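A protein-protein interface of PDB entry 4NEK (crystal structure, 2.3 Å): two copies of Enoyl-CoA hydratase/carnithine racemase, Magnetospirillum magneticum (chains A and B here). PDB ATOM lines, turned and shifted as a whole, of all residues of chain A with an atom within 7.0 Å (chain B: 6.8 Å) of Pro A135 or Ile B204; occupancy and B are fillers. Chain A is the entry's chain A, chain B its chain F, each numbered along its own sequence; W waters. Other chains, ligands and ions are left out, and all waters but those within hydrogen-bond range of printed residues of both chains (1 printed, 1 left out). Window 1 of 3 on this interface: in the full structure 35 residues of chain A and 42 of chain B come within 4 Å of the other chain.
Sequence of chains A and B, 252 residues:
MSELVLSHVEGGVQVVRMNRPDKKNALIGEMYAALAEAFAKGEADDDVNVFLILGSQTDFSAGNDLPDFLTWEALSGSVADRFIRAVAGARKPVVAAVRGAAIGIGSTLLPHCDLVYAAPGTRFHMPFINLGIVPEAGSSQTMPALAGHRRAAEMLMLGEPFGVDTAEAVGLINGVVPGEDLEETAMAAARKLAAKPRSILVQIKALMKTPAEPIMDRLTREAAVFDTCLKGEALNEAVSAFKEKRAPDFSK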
ATOM      1  N   LEU A  75      21.300 -12.145  14.633  1.00  0.00           N
ATOM      2  CA  LEU A  75      21.892 -11.475  13.495  1.00  0.00           C
ATOM      3  C   LEU A  75      22.289 -10.064  13.891  1.00  0.00           C
ATOM      4  O   LEU A  75      23.387  -9.641  13.599  1.00  0.00           O
ATOM      5  CB  LEU A  75      20.926 -11.466  12.317  1.00  0.00           C
ATOM      6  CG  LEU A  75      21.400 -10.671  11.096  1.00  0.00           C
ATOM      7  CD1 LEU A  75      22.699 -11.204  10.550  1.00  0.00           C
ATOM      8  CD2 LEU A  75      20.329 -10.629  10.022  1.00  0.00           C
ATOM      9  N   THR A 108      22.097 -11.473  -1.754  1.00  0.00           N
ATOM     10  CA  THR A 108      21.468 -10.291  -1.163  1.00  0.00           C
ATOM     11  C   THR A 108      22.439  -9.154  -0.963  1.00  0.00           C
ATOM     12  O   THR A 108      22.052  -8.020  -0.684  1.00  0.00           O
ATOM     13  CB  THR A 108      20.858 -10.592   0.196  1.00  0.00           C
ATOM     14  OG1 THR A 108      21.859 -11.116   1.072  1.00  0.00           O
ATOM     15  CG2 THR A 108      19.741 -11.601   0.045  1.00  0.00           C
ATOM     16  N   MET A 126      17.606 -17.053  -2.765  1.00  0.00           N
ATOM     17  CA  MET A 126      17.340 -16.516  -1.426  1.00  0.00           C
ATOM     18  C   MET A 126      16.375 -17.401  -0.703  1.00  0.00           C
ATOM     19  O   MET A 126      15.208 -17.050  -0.557  1.00  0.00           O
ATOM     20  CB  MET A 126      16.756 -15.138  -1.610  1.00  0.00           C
ATOM     21  CG  MET A 126      17.893 -14.245  -2.084  1.00  0.00           C
ATOM     22  SD  MET A 126      17.174 -12.556  -2.813  1.00  0.00           S
ATOM     23  CE  MET A 126      18.391 -12.164  -4.307  1.00  0.00           C
ATOM     24  N   PHE A 128      15.628 -18.199   2.391  1.00  0.00           N
ATOM     25  CA  PHE A 128      15.255 -17.888   3.769  1.00  0.00           C
ATOM     26  C   PHE A 128      13.951 -18.519   4.214  1.00  0.00           C
ATOM     27  O   PHE A 128      13.921 -19.199   5.212  1.00  0.00           O
ATOM     28  CB  PHE A 128      15.155 -16.379   3.964  1.00  0.00           C
ATOM     29  CG  PHE A 128      16.366 -15.658   3.490  1.00  0.00           C
ATOM     30  CD1 PHE A 128      17.508 -15.679   4.242  1.00  0.00           C
ATOM     31  CD2 PHE A 128      16.370 -15.012   2.258  1.00  0.00           C
ATOM     32  CE1 PHE A 128      18.648 -15.034   3.803  1.00  0.00           C
ATOM     33  CE2 PHE A 128      17.506 -14.357   1.803  1.00  0.00           C
ATOM     34  CZ  PHE A 128      18.650 -14.374   2.586  1.00  0.00           C
ATOM     35  N   ILE A 129      12.889 -18.340   3.436  1.00  0.00           N
ATOM     36  CA  ILE A 129      11.617 -18.934   3.777  1.00  0.00           C
ATOM     37  C   ILE A 129      11.686 -20.449   4.011  1.00  0.00           C
ATOM     38  O   ILE A 129      11.004 -20.968   4.895  1.00  0.00           O
ATOM     39  CB  ILE A 129      10.523 -18.633   2.726  1.00  0.00           C
ATOM     40  CG1 ILE A 129       9.139 -19.136   3.187  1.00  0.00           C
ATOM     41  CG2 ILE A 129      10.831 -19.252   1.376  1.00  0.00           C
ATOM     42  CD1 ILE A 129       8.695 -18.619   4.529  1.00  0.00           C
ATOM     43  N   ASN A 130      12.484 -21.152   3.228  1.00  0.00           N
ATOM     44  CA  ASN A 130      12.592 -22.608   3.404  1.00  0.00           C
ATOM     45  C   ASN A 130      13.395 -23.003   4.594  1.00  0.00           C
ATOM     46  O   ASN A 130      13.434 -24.161   4.920  1.00  0.00           O
ATOM     47  CB  ASN A 130      13.225 -23.256   2.183  1.00  0.00           C
ATOM     48  CG  ASN A 130      12.415 -23.050   0.953  1.00  0.00           C
ATOM     49  OD1 ASN A 130      12.961 -22.931  -0.132  1.00  0.00           O
ATOM     50  ND2 ASN A 130      11.115 -22.994   1.096  1.00  0.00           N
ATOM     51  N   GLY A 132      12.797 -21.297   7.463  1.00  0.00           N
ATOM     52  CA  GLY A 132      12.049 -20.687   8.555  1.00  0.00           C
ATOM     53  C   GLY A 132      12.603 -19.360   9.029  1.00  0.00           C
ATOM     54  O   GLY A 132      12.393 -18.955  10.182  1.00  0.00           O
ATOM     55  N   ILE A 133      13.292 -18.653   8.157  1.00  0.00           N
ATOM     56  CA  ILE A 133      13.777 -17.347   8.531  1.00  0.00           C
ATOM     57  C   ILE A 133      13.399 -16.282   7.518  1.00  0.00           C
ATOM     58  O   ILE A 133      12.793 -16.572   6.501  1.00  0.00           O
ATOM     59  CB  ILE A 133      15.295 -17.392   8.754  1.00  0.00           C
ATOM     60  CG1 ILE A 133      16.009 -17.794   7.475  1.00  0.00           C
ATOM     61  CG2 ILE A 133      15.630 -18.399   9.861  1.00  0.00           C
ATOM     62  CD1 ILE A 133      17.527 -17.782   7.605  1.00  0.00           C
ATOM     63  N   VAL A 134      13.768 -15.037   7.802  1.00  0.00           N
ATOM     64  CA  VAL A 134      13.473 -13.945   6.905  1.00  0.00           C
ATOM     65  C   VAL A 134      14.710 -13.469   6.156  1.00  0.00           C
ATOM     66  O   VAL A 134      15.840 -13.701   6.596  1.00  0.00           O
ATOM     67  CB  VAL A 134      12.814 -12.760   7.638  1.00  0.00           C
ATOM     68  CG1 VAL A 134      11.575 -13.240   8.378  1.00  0.00           C
ATOM     69  CG2 VAL A 134      13.799 -12.025   8.569  1.00  0.00           C
ATOM     70  N   PRO A 135      14.496 -12.787   5.019  1.00  0.00           N
ATOM     71  CA  PRO A 135      15.589 -12.163   4.310  1.00  0.00           C
ATOM     72  C   PRO A 135      16.286 -11.021   5.036  1.00  0.00           C
ATOM     73  O   PRO A 135      15.715 -10.288   5.822  1.00  0.00           O
ATOM     74  CB  PRO A 135      14.923 -11.564   3.088  1.00  0.00           C
ATOM     75  CG  PRO A 135      13.590 -12.166   3.023  1.00  0.00           C
ATOM     76  CD  PRO A 135      13.215 -12.390   4.437  1.00  0.00           C
ATOM     77  N   GLU A 136      17.537 -10.912   4.698  1.00  0.00           N
ATOM     78  CA  GLU A 136      18.495 -10.128   5.382  1.00  0.00           C
ATOM     79  C   GLU A 136      19.069  -9.158   4.341  1.00  0.00           C
ATOM     80  O   GLU A 136      18.717  -9.192   3.156  1.00  0.00           O
ATOM     81  CB  GLU A 136      19.626 -11.090   5.844  1.00  0.00           C
ATOM     82  CG  GLU A 136      20.542 -11.503   4.663  1.00  0.00           C
ATOM     83  CD  GLU A 136      21.363 -12.766   4.872  1.00  0.00           C
ATOM     84  OE1 GLU A 136      21.306 -13.379   5.976  1.00  0.00           O
ATOM     85  OE2 GLU A 136      22.094 -13.152   3.922  1.00  0.00           O
ATOM     86  N   ALA A 137      20.026  -8.373   4.806  1.00  0.00           N
ATOM     87  CA  ALA A 137      20.835  -7.511   3.994  1.00  0.00           C
ATOM     88  C   ALA A 137      20.014  -6.520   3.195  1.00  0.00           C
ATOM     89  O   ALA A 137      20.509  -5.982   2.211  1.00  0.00           O
ATOM     90  CB  ALA A 137      21.775  -8.319   3.089  1.00  0.00           C
ATOM     91  N   GLY A 138      18.801  -6.205   3.658  1.00  0.00           N
ATOM     92  CA  GLY A 138      17.931  -5.222   3.009  1.00  0.00           C
ATOM     93  C   GLY A 138      17.173  -5.733   1.800  1.00  0.00           C
ATOM     94  O   GLY A 138      16.516  -4.954   1.099  1.00  0.00           O
ATOM     95  N   SER A 139      17.209  -7.044   1.580  1.00  0.00           N
ATOM     96  CA  SER A 139      16.595  -7.619   0.393  1.00  0.00           C
ATOM     97  C   SER A 139      15.082  -7.478   0.358  1.00  0.00           C
ATOM     98  O   SER A 139      14.510  -7.352  -0.723  1.00  0.00           O
ATOM     99  CB  SER A 139      16.995  -9.087   0.231  1.00  0.00           C
ATOM    100  OG  SER A 139      16.752  -9.764   1.408  1.00  0.00           O
ATOM    101  N   SER A 140      14.440  -7.455   1.530  1.00  0.00           N
ATOM    102  CA  SER A 140      13.007  -7.123   1.614  1.00  0.00           C
ATOM    103  C   SER A 140      12.659  -5.761   1.048  1.00  0.00           C
ATOM    104  O   SER A 140      11.537  -5.539   0.662  1.00  0.00           O
ATOM    105  CB  SER A 140      12.504  -7.163   3.072  1.00  0.00           C
ATOM    106  OG  SER A 140      12.994  -6.053   3.845  1.00  0.00           O
ATOM    107  N   HIS A 149       7.035  -6.213  -6.926  1.00  0.00           N
ATOM    108  CA  HIS A 149       6.651  -7.090  -5.844  1.00  0.00           C
ATOM    109  C   HIS A 149       6.444  -8.551  -6.280  1.00  0.00           C
ATOM    110  O   HIS A 149       6.779  -9.489  -5.525  1.00  0.00           O
ATOM    111  CB  HIS A 149       5.402  -6.558  -5.177  1.00  0.00           C
ATOM    112  CG  HIS A 149       4.980  -7.385  -4.022  1.00  0.00           C
ATOM    113  ND1 HIS A 149       5.601  -7.315  -2.799  1.00  0.00           N
ATOM    114  CD2 HIS A 149       4.051  -8.368  -3.919  1.00  0.00           C
ATOM    115  CE1 HIS A 149       5.055  -8.200  -1.976  1.00  0.00           C
ATOM    116  NE2 HIS A 149       4.125  -8.866  -2.638  1.00  0.00           N
ATOM    117  N   LEU A 156      11.541 -14.459  -2.770  1.00  0.00           N
ATOM    118  CA  LEU A 156      11.510 -14.397  -1.322  1.00  0.00           C
ATOM    119  C   LEU A 156      10.378 -15.193  -0.636  1.00  0.00           C
ATOM    120  O   LEU A 156      10.557 -15.686   0.473  1.00  0.00           O
ATOM    121  CB  LEU A 156      11.389 -12.954  -0.884  1.00  0.00           C
ATOM    122  CG  LEU A 156      12.488 -12.043  -1.381  1.00  0.00           C
ATOM    123  CD1 LEU A 156      12.323 -10.647  -0.843  1.00  0.00           C
ATOM    124  CD2 LEU A 156      13.842 -12.589  -0.977  1.00  0.00           C
ATOM    125  N   MET A 157       9.227 -15.299  -1.280  1.00  0.00           N
ATOM    126  CA  MET A 157       8.113 -15.958  -0.671  1.00  0.00           C
ATOM    127  C   MET A 157       8.060 -17.382  -1.144  1.00  0.00           C
ATOM    128  O   MET A 157       7.818 -18.278  -0.324  1.00  0.00           O
ATOM    129  CB  MET A 157       6.854 -15.161  -0.936  1.00  0.00           C
ATOM    130  CG  MET A 157       6.852 -13.851  -0.111  1.00  0.00           C
ATOM    131  SD  MET A 157       5.244 -12.715  -0.532  1.00  0.00           S
ATOM    132  CE  MET A 157       3.885 -14.016   0.036  1.00  0.00           C
ATOM    133  N   SER B 199       3.706 -18.359   9.633  1.00  0.00           N
ATOM    134  CA  SER B 199       4.024 -17.216  10.475  1.00  0.00           C
ATOM    135  C   SER B 199       5.229 -16.511   9.917  1.00  0.00           C
ATOM    136  O   SER B 199       5.291 -15.298   9.943  1.00  0.00           O
ATOM    137  CB  SER B 199       4.284 -17.659  11.881  1.00  0.00           C
ATOM    138  OG  SER B 199       5.254 -18.688  11.826  1.00  0.00           O
ATOM    139  N   ILE B 200       6.171 -17.257   9.371  1.00  0.00           N
ATOM    140  CA  ILE B 200       7.312 -16.626   8.727  1.00  0.00           C
ATOM    141  C   ILE B 200       6.919 -15.950   7.419  1.00  0.00           C
ATOM    142  O   ILE B 200       7.333 -14.811   7.131  1.00  0.00           O
ATOM    143  CB  ILE B 200       8.376 -17.644   8.380  1.00  0.00           C
ATOM    144  CG1 ILE B 200       8.761 -18.525   9.605  1.00  0.00           C
ATOM    145  CG2 ILE B 200       9.602 -16.930   7.833  1.00  0.00           C
ATOM    146  CD1 ILE B 200       9.232 -17.734  10.813  1.00  0.00           C
ATOM    147  N   LEU B 201       6.158 -16.654   6.605  1.00  0.00           N
ATOM    148  CA  LEU B 201       5.763 -16.128   5.306  1.00  0.00           C
ATOM    149  C   LEU B 201       5.051 -14.782   5.405  1.00  0.00           C
ATOM    150  O   LEU B 201       5.313 -13.855   4.646  1.00  0.00           O
ATOM    151  CB  LEU B 201       4.836 -17.095   4.616  1.00  0.00           C
ATOM    152  CG  LEU B 201       4.596 -16.797   3.150  1.00  0.00           C
ATOM    153  CD1 LEU B 201       5.874 -16.700   2.349  1.00  0.00           C
ATOM    154  CD2 LEU B 201       3.766 -17.896   2.540  1.00  0.00           C
ATOM    155  N   VAL B 202       4.181 -14.670   6.384  1.00  0.00           N
ATOM    156  CA  VAL B 202       3.489 -13.444   6.647  1.00  0.00           C
ATOM    157  C   VAL B 202       4.461 -12.314   7.004  1.00  0.00           C
ATOM    158  O   VAL B 202       4.247 -11.158   6.634  1.00  0.00           O
ATOM    159  CB  VAL B 202       2.467 -13.709   7.767  1.00  0.00           C
ATOM    160  CG1 VAL B 202       2.056 -12.457   8.522  1.00  0.00           C
ATOM    161  CG2 VAL B 202       1.243 -14.379   7.178  1.00  0.00           C
ATOM    162  N   GLN B 203       5.507 -12.626   7.763  1.00  0.00           N
ATOM    163  CA  GLN B 203       6.479 -11.613   8.161  1.00  0.00           C
ATOM    164  C   GLN B 203       7.272 -11.135   6.937  1.00  0.00           C
ATOM    165  O   GLN B 203       7.593  -9.963   6.797  1.00  0.00           O
ATOM    166  CB  GLN B 203       7.461 -12.198   9.171  1.00  0.00           C
ATOM    167  CG  GLN B 203       6.907 -12.535  10.554  1.00  0.00           C
ATOM    168  CD  GLN B 203       6.419 -11.303  11.251  1.00  0.00           C
ATOM    169  OE1 GLN B 203       7.124 -10.283  11.319  1.00  0.00           O
ATOM    170  NE2 GLN B 203       5.156 -11.329  11.678  1.00  0.00           N
ATOM    171  N   ILE B 204       7.594 -12.071   6.060  1.00  0.00           N
ATOM    172  CA  ILE B 204       8.291 -11.730   4.827  1.00  0.00           C
ATOM    173  C   ILE B 204       7.435 -10.813   3.971  1.00  0.00           C
ATOM    174  O   ILE B 204       7.912  -9.784   3.509  1.00  0.00           O
ATOM    175  CB  ILE B 204       8.661 -12.977   4.049  1.00  0.00           C
ATOM    176  CG1 ILE B 204       9.758 -13.722   4.826  1.00  0.00           C
ATOM    177  CG2 ILE B 204       9.155 -12.622   2.660  1.00  0.00           C
ATOM    178  CD1 ILE B 204      10.173 -15.039   4.211  1.00  0.00           C
ATOM    179  N   LYS B 205       6.162 -11.144   3.820  1.00  0.00           N
ATOM    180  CA  LYS B 205       5.279 -10.286   3.073  1.00  0.00           C
ATOM    181  C   LYS B 205       5.184  -8.899   3.684  1.00  0.00           C
ATOM    182  O   LYS B 205       5.239  -7.891   2.987  1.00  0.00           O
ATOM    183  CB  LYS B 205       3.910 -10.891   2.952  1.00  0.00           C
ATOM    184  CG  LYS B 205       2.940  -9.959   2.238  1.00  0.00           C
ATOM    185  CD  LYS B 205       1.646 -10.655   1.840  1.00  0.00           C
ATOM    186  CE  LYS B 205       0.658  -9.622   1.407  1.00  0.00           C
ATOM    187  NZ  LYS B 205      -0.562 -10.198   0.778  1.00  0.00           N
ATOM    188  N   ALA B 206       5.091  -8.844   5.003  1.00  0.00           N
ATOM    189  CA  ALA B 206       4.943  -7.539   5.686  1.00  0.00           C
ATOM    190  C   ALA B 206       6.196  -6.698   5.509  1.00  0.00           C
ATOM    191  O   ALA B 206       6.125  -5.496   5.264  1.00  0.00           O
ATOM    192  CB  ALA B 206       4.633  -7.729   7.175  1.00  0.00           C
ATOM    193  N   LEU B 207       7.345  -7.339   5.609  1.00  0.00           N
ATOM    194  CA  LEU B 207       8.574  -6.613   5.335  1.00  0.00           C
ATOM    195  C   LEU B 207       8.609  -6.107   3.909  1.00  0.00           C
ATOM    196  O   LEU B 207       8.951  -4.935   3.651  1.00  0.00           O
ATOM    197  CB  LEU B 207       9.784  -7.498   5.588  1.00  0.00           C
ATOM    198  CG  LEU B 207      10.103  -7.687   7.052  1.00  0.00           C
ATOM    199  CD1 LEU B 207      11.088  -8.847   7.204  1.00  0.00           C
ATOM    200  CD2 LEU B 207      10.665  -6.422   7.710  1.00  0.00           C
ATOM    201  N   MET B 208       8.310  -6.990   2.973  1.00  0.00           N
ATOM    202  CA  MET B 208       8.351  -6.612   1.558  1.00  0.00           C
ATOM    203  C   MET B 208       7.458  -5.438   1.285  1.00  0.00           C
ATOM    204  O   MET B 208       7.808  -4.581   0.487  1.00  0.00           O
ATOM    205  CB  MET B 208       7.868  -7.699   0.635  1.00  0.00           C
ATOM    206  CG  MET B 208       8.964  -8.729   0.509  1.00  0.00           C
ATOM    207  SD  MET B 208       8.253 -10.267  -0.484  1.00  0.00           S
ATOM    208  CE  MET B 208       8.230  -9.516  -2.307  1.00  0.00           C
ATOM    209  N   LYS B 209       6.343  -5.365   1.992  1.00  0.00           N
ATOM    210  CA  LYS B 209       5.389  -4.290   1.800  1.00  0.00           C
ATOM    211  C   LYS B 209       5.530  -3.093   2.747  1.00  0.00           C
ATOM    212  O   LYS B 209       4.719  -2.182   2.709  1.00  0.00           O
ATOM    213  CB  LYS B 209       4.010  -4.859   1.898  1.00  0.00           C
ATOM    214  CG  LYS B 209       3.770  -5.804   0.734  1.00  0.00           C
ATOM    215  CD  LYS B 209       2.384  -6.376   0.690  1.00  0.00           C
ATOM    216  CE  LYS B 209       1.397  -5.294   0.339  1.00  0.00           C
ATOM    217  NZ  LYS B 209       0.071  -5.899   0.005  1.00  0.00           N
ATOM    218  N   GLU B 222      14.993  -5.738   9.594  1.00  0.00           N
ATOM    219  CA  GLU B 222      14.989  -7.135   9.150  1.00  0.00           C
ATOM    220  C   GLU B 222      15.639  -7.961  10.184  1.00  0.00           C
ATOM    221  O   GLU B 222      15.147  -9.029  10.528  1.00  0.00           O
ATOM    222  CB  GLU B 222      15.760  -7.328   7.846  1.00  0.00           C
ATOM    223  CG  GLU B 222      15.060  -6.801   6.614  1.00  0.00           C
ATOM    224  CD  GLU B 222      15.928  -6.855   5.349  1.00  0.00           C
ATOM    225  OE1 GLU B 222      17.176  -6.948   5.483  1.00  0.00           O
ATOM    226  OE2 GLU B 222      15.358  -6.833   4.214  1.00  0.00           O
ATOM    227  N   ALA B 223      16.737  -7.438  10.712  1.00  0.00           N
ATOM    228  CA  ALA B 223      17.517  -8.170  11.708  1.00  0.00           C
ATOM    229  C   ALA B 223      16.720  -8.433  12.993  1.00  0.00           C
ATOM    230  O   ALA B 223      16.773  -9.515  13.536  1.00  0.00           O
ATOM    231  CB  ALA B 223      18.810  -7.446  12.010  1.00  0.00           C
ATOM    232  N   VAL B 225      13.497  -8.833  13.260  1.00  0.00           N
ATOM    233  CA  VAL B 225      12.612  -9.939  12.982  1.00  0.00           C
ATOM    234  C   VAL B 225      13.423 -11.239  12.911  1.00  0.00           C
ATOM    235  O   VAL B 225      13.040 -12.262  13.484  1.00  0.00           O
ATOM    236  CB  VAL B 225      11.865  -9.733  11.657  1.00  0.00           C
ATOM    237  CG1 VAL B 225      10.988 -10.931  11.342  1.00  0.00           C
ATOM    238  CG2 VAL B 225      11.022  -8.471  11.725  1.00  0.00           C
ATOM    239  N   PHE B 226      14.528 -11.180  12.193  1.00  0.00           N
ATOM    240  CA  PHE B 226      15.355 -12.331  11.956  1.00  0.00           C
ATOM    241  C   PHE B 226      15.785 -12.973  13.262  1.00  0.00           C
ATOM    242  O   PHE B 226      15.755 -14.207  13.398  1.00  0.00           O
ATOM    243  CB  PHE B 226      16.569 -11.887  11.151  1.00  0.00           C
ATOM    244  CG  PHE B 226      17.433 -13.016  10.614  1.00  0.00           C
ATOM    245  CD1 PHE B 226      18.339 -13.675  11.435  1.00  0.00           C
ATOM    246  CD2 PHE B 226      17.382 -13.355   9.276  1.00  0.00           C
ATOM    247  CE1 PHE B 226      19.155 -14.670  10.936  1.00  0.00           C
ATOM    248  CE2 PHE B 226      18.191 -14.349   8.767  1.00  0.00           C
ATOM    249  CZ  PHE B 226      19.084 -15.017   9.601  1.00  0.00           C
HETATM  250  O   HOH W   1       6.594  -4.884  -2.037  1.00  0.00           O
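Of the printed residues of chain B, Gly A138 touches Glu B222 (2.6 Å). Of the printed residues of chain A, Ile B204 touches Ile A129, Ile A133, Pro A135, Leu A156 and Met A157. Printed residues of chain A within 4 Å of Leu B207: Ser A140 (3.7 Å). Of the printed residues of chain A, Met B208 touches Ser A140, His A149 and Met A157. Ala B223 touches none of the printed residues of chain A. The nearest residue of chain B that does not touch Pro A135 is Phe B226 (4.9 Å). The nearest printed residue of chain A that does not touch Ile B204 is Val A134 (4.02 Å). The nearest printed residue of chain A that does not touch Phe B226 is Glu A136 (4.3 Å).
Among the printed residues, merely in contact across the chains: Val A134 with Phe B226, Glu A136 with Glu B222, Gly A132 with Ile B200, His A149 with Met B208, Pro A135 with Glu B222, Ile A133 with Ile B200, Ser A140 with Met B208, Leu A75 with Phe B226, Met A157 with Leu B201, Ile A133 with Phe B226, Ser A140 with Leu B207, Pro A135 with Ile B204, Ile A133 with Ile B204, Val A134 with Val B225, Met A157 with Ile B204, Leu A156 with Ile B204, Ile A129 with Ile B200, Ile A129 with Leu B201, Val A134 with Glu B222, His A149 with Lys B209, Met A157 with Met B208 and Ile A129 with Ile B204.
N of Ala A137 is in hydrogen-bond range of OE1 of Glu B222 (3.3 Å). N of Gly A138 sits at hydrogen-bond distance from OE1 of Glu B222, at 2.6 Å. The backbone NH (N) of Ser A139 sits at hydrogen-bond distance from the side-chain carboxylate (OE2) of Glu B222 (3.2 Å). The side-chain hydroxyl (OG) of Ser A140 is in hydrogen-bond range of the side-chain carboxylate (OE2) of Glu B222.
O of Phe A128 is in hydrogen-bond range of N of Ile A133 (3.1 Å). The backbone carbonyl oxygen (O) of Glu A136 is in hydrogen-bond range of the side-chain hydroxyl (OG) of Ser A139 (2.7 Å).
Hydrophobic or aromatic side chains of chain B within 4 Å of the printed part of chain A: Ile B200, Leu B201, Ile B204, Leu B207, Met B208, Val B225 and Phe B226. Of the 18 printed residues of chain A, 14 touch a printed residue of chain B. Hydrophobic or aromatic side chains of chain A that line the printed part of chain B: Leu A75, Ile A129, Ile A133, Val A134, Pro A135, His A149 and Met A157. Among the printed residues, 26 pairs touch across the chains. Among the printed residues, no Asp or Glu carboxylate lies within 4 Å of a Lys or Arg side-chain nitrogen of the other chain.
Water W1 lies within hydrogen-bond range of ND1 of His A149 (2.7 Å) and O of Met B208 (2.8 Å).
No position is printed for both chains. Of the 26 pairs that touch across the chains among the printed residues, none has its exchanged pair printed and touching as well.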
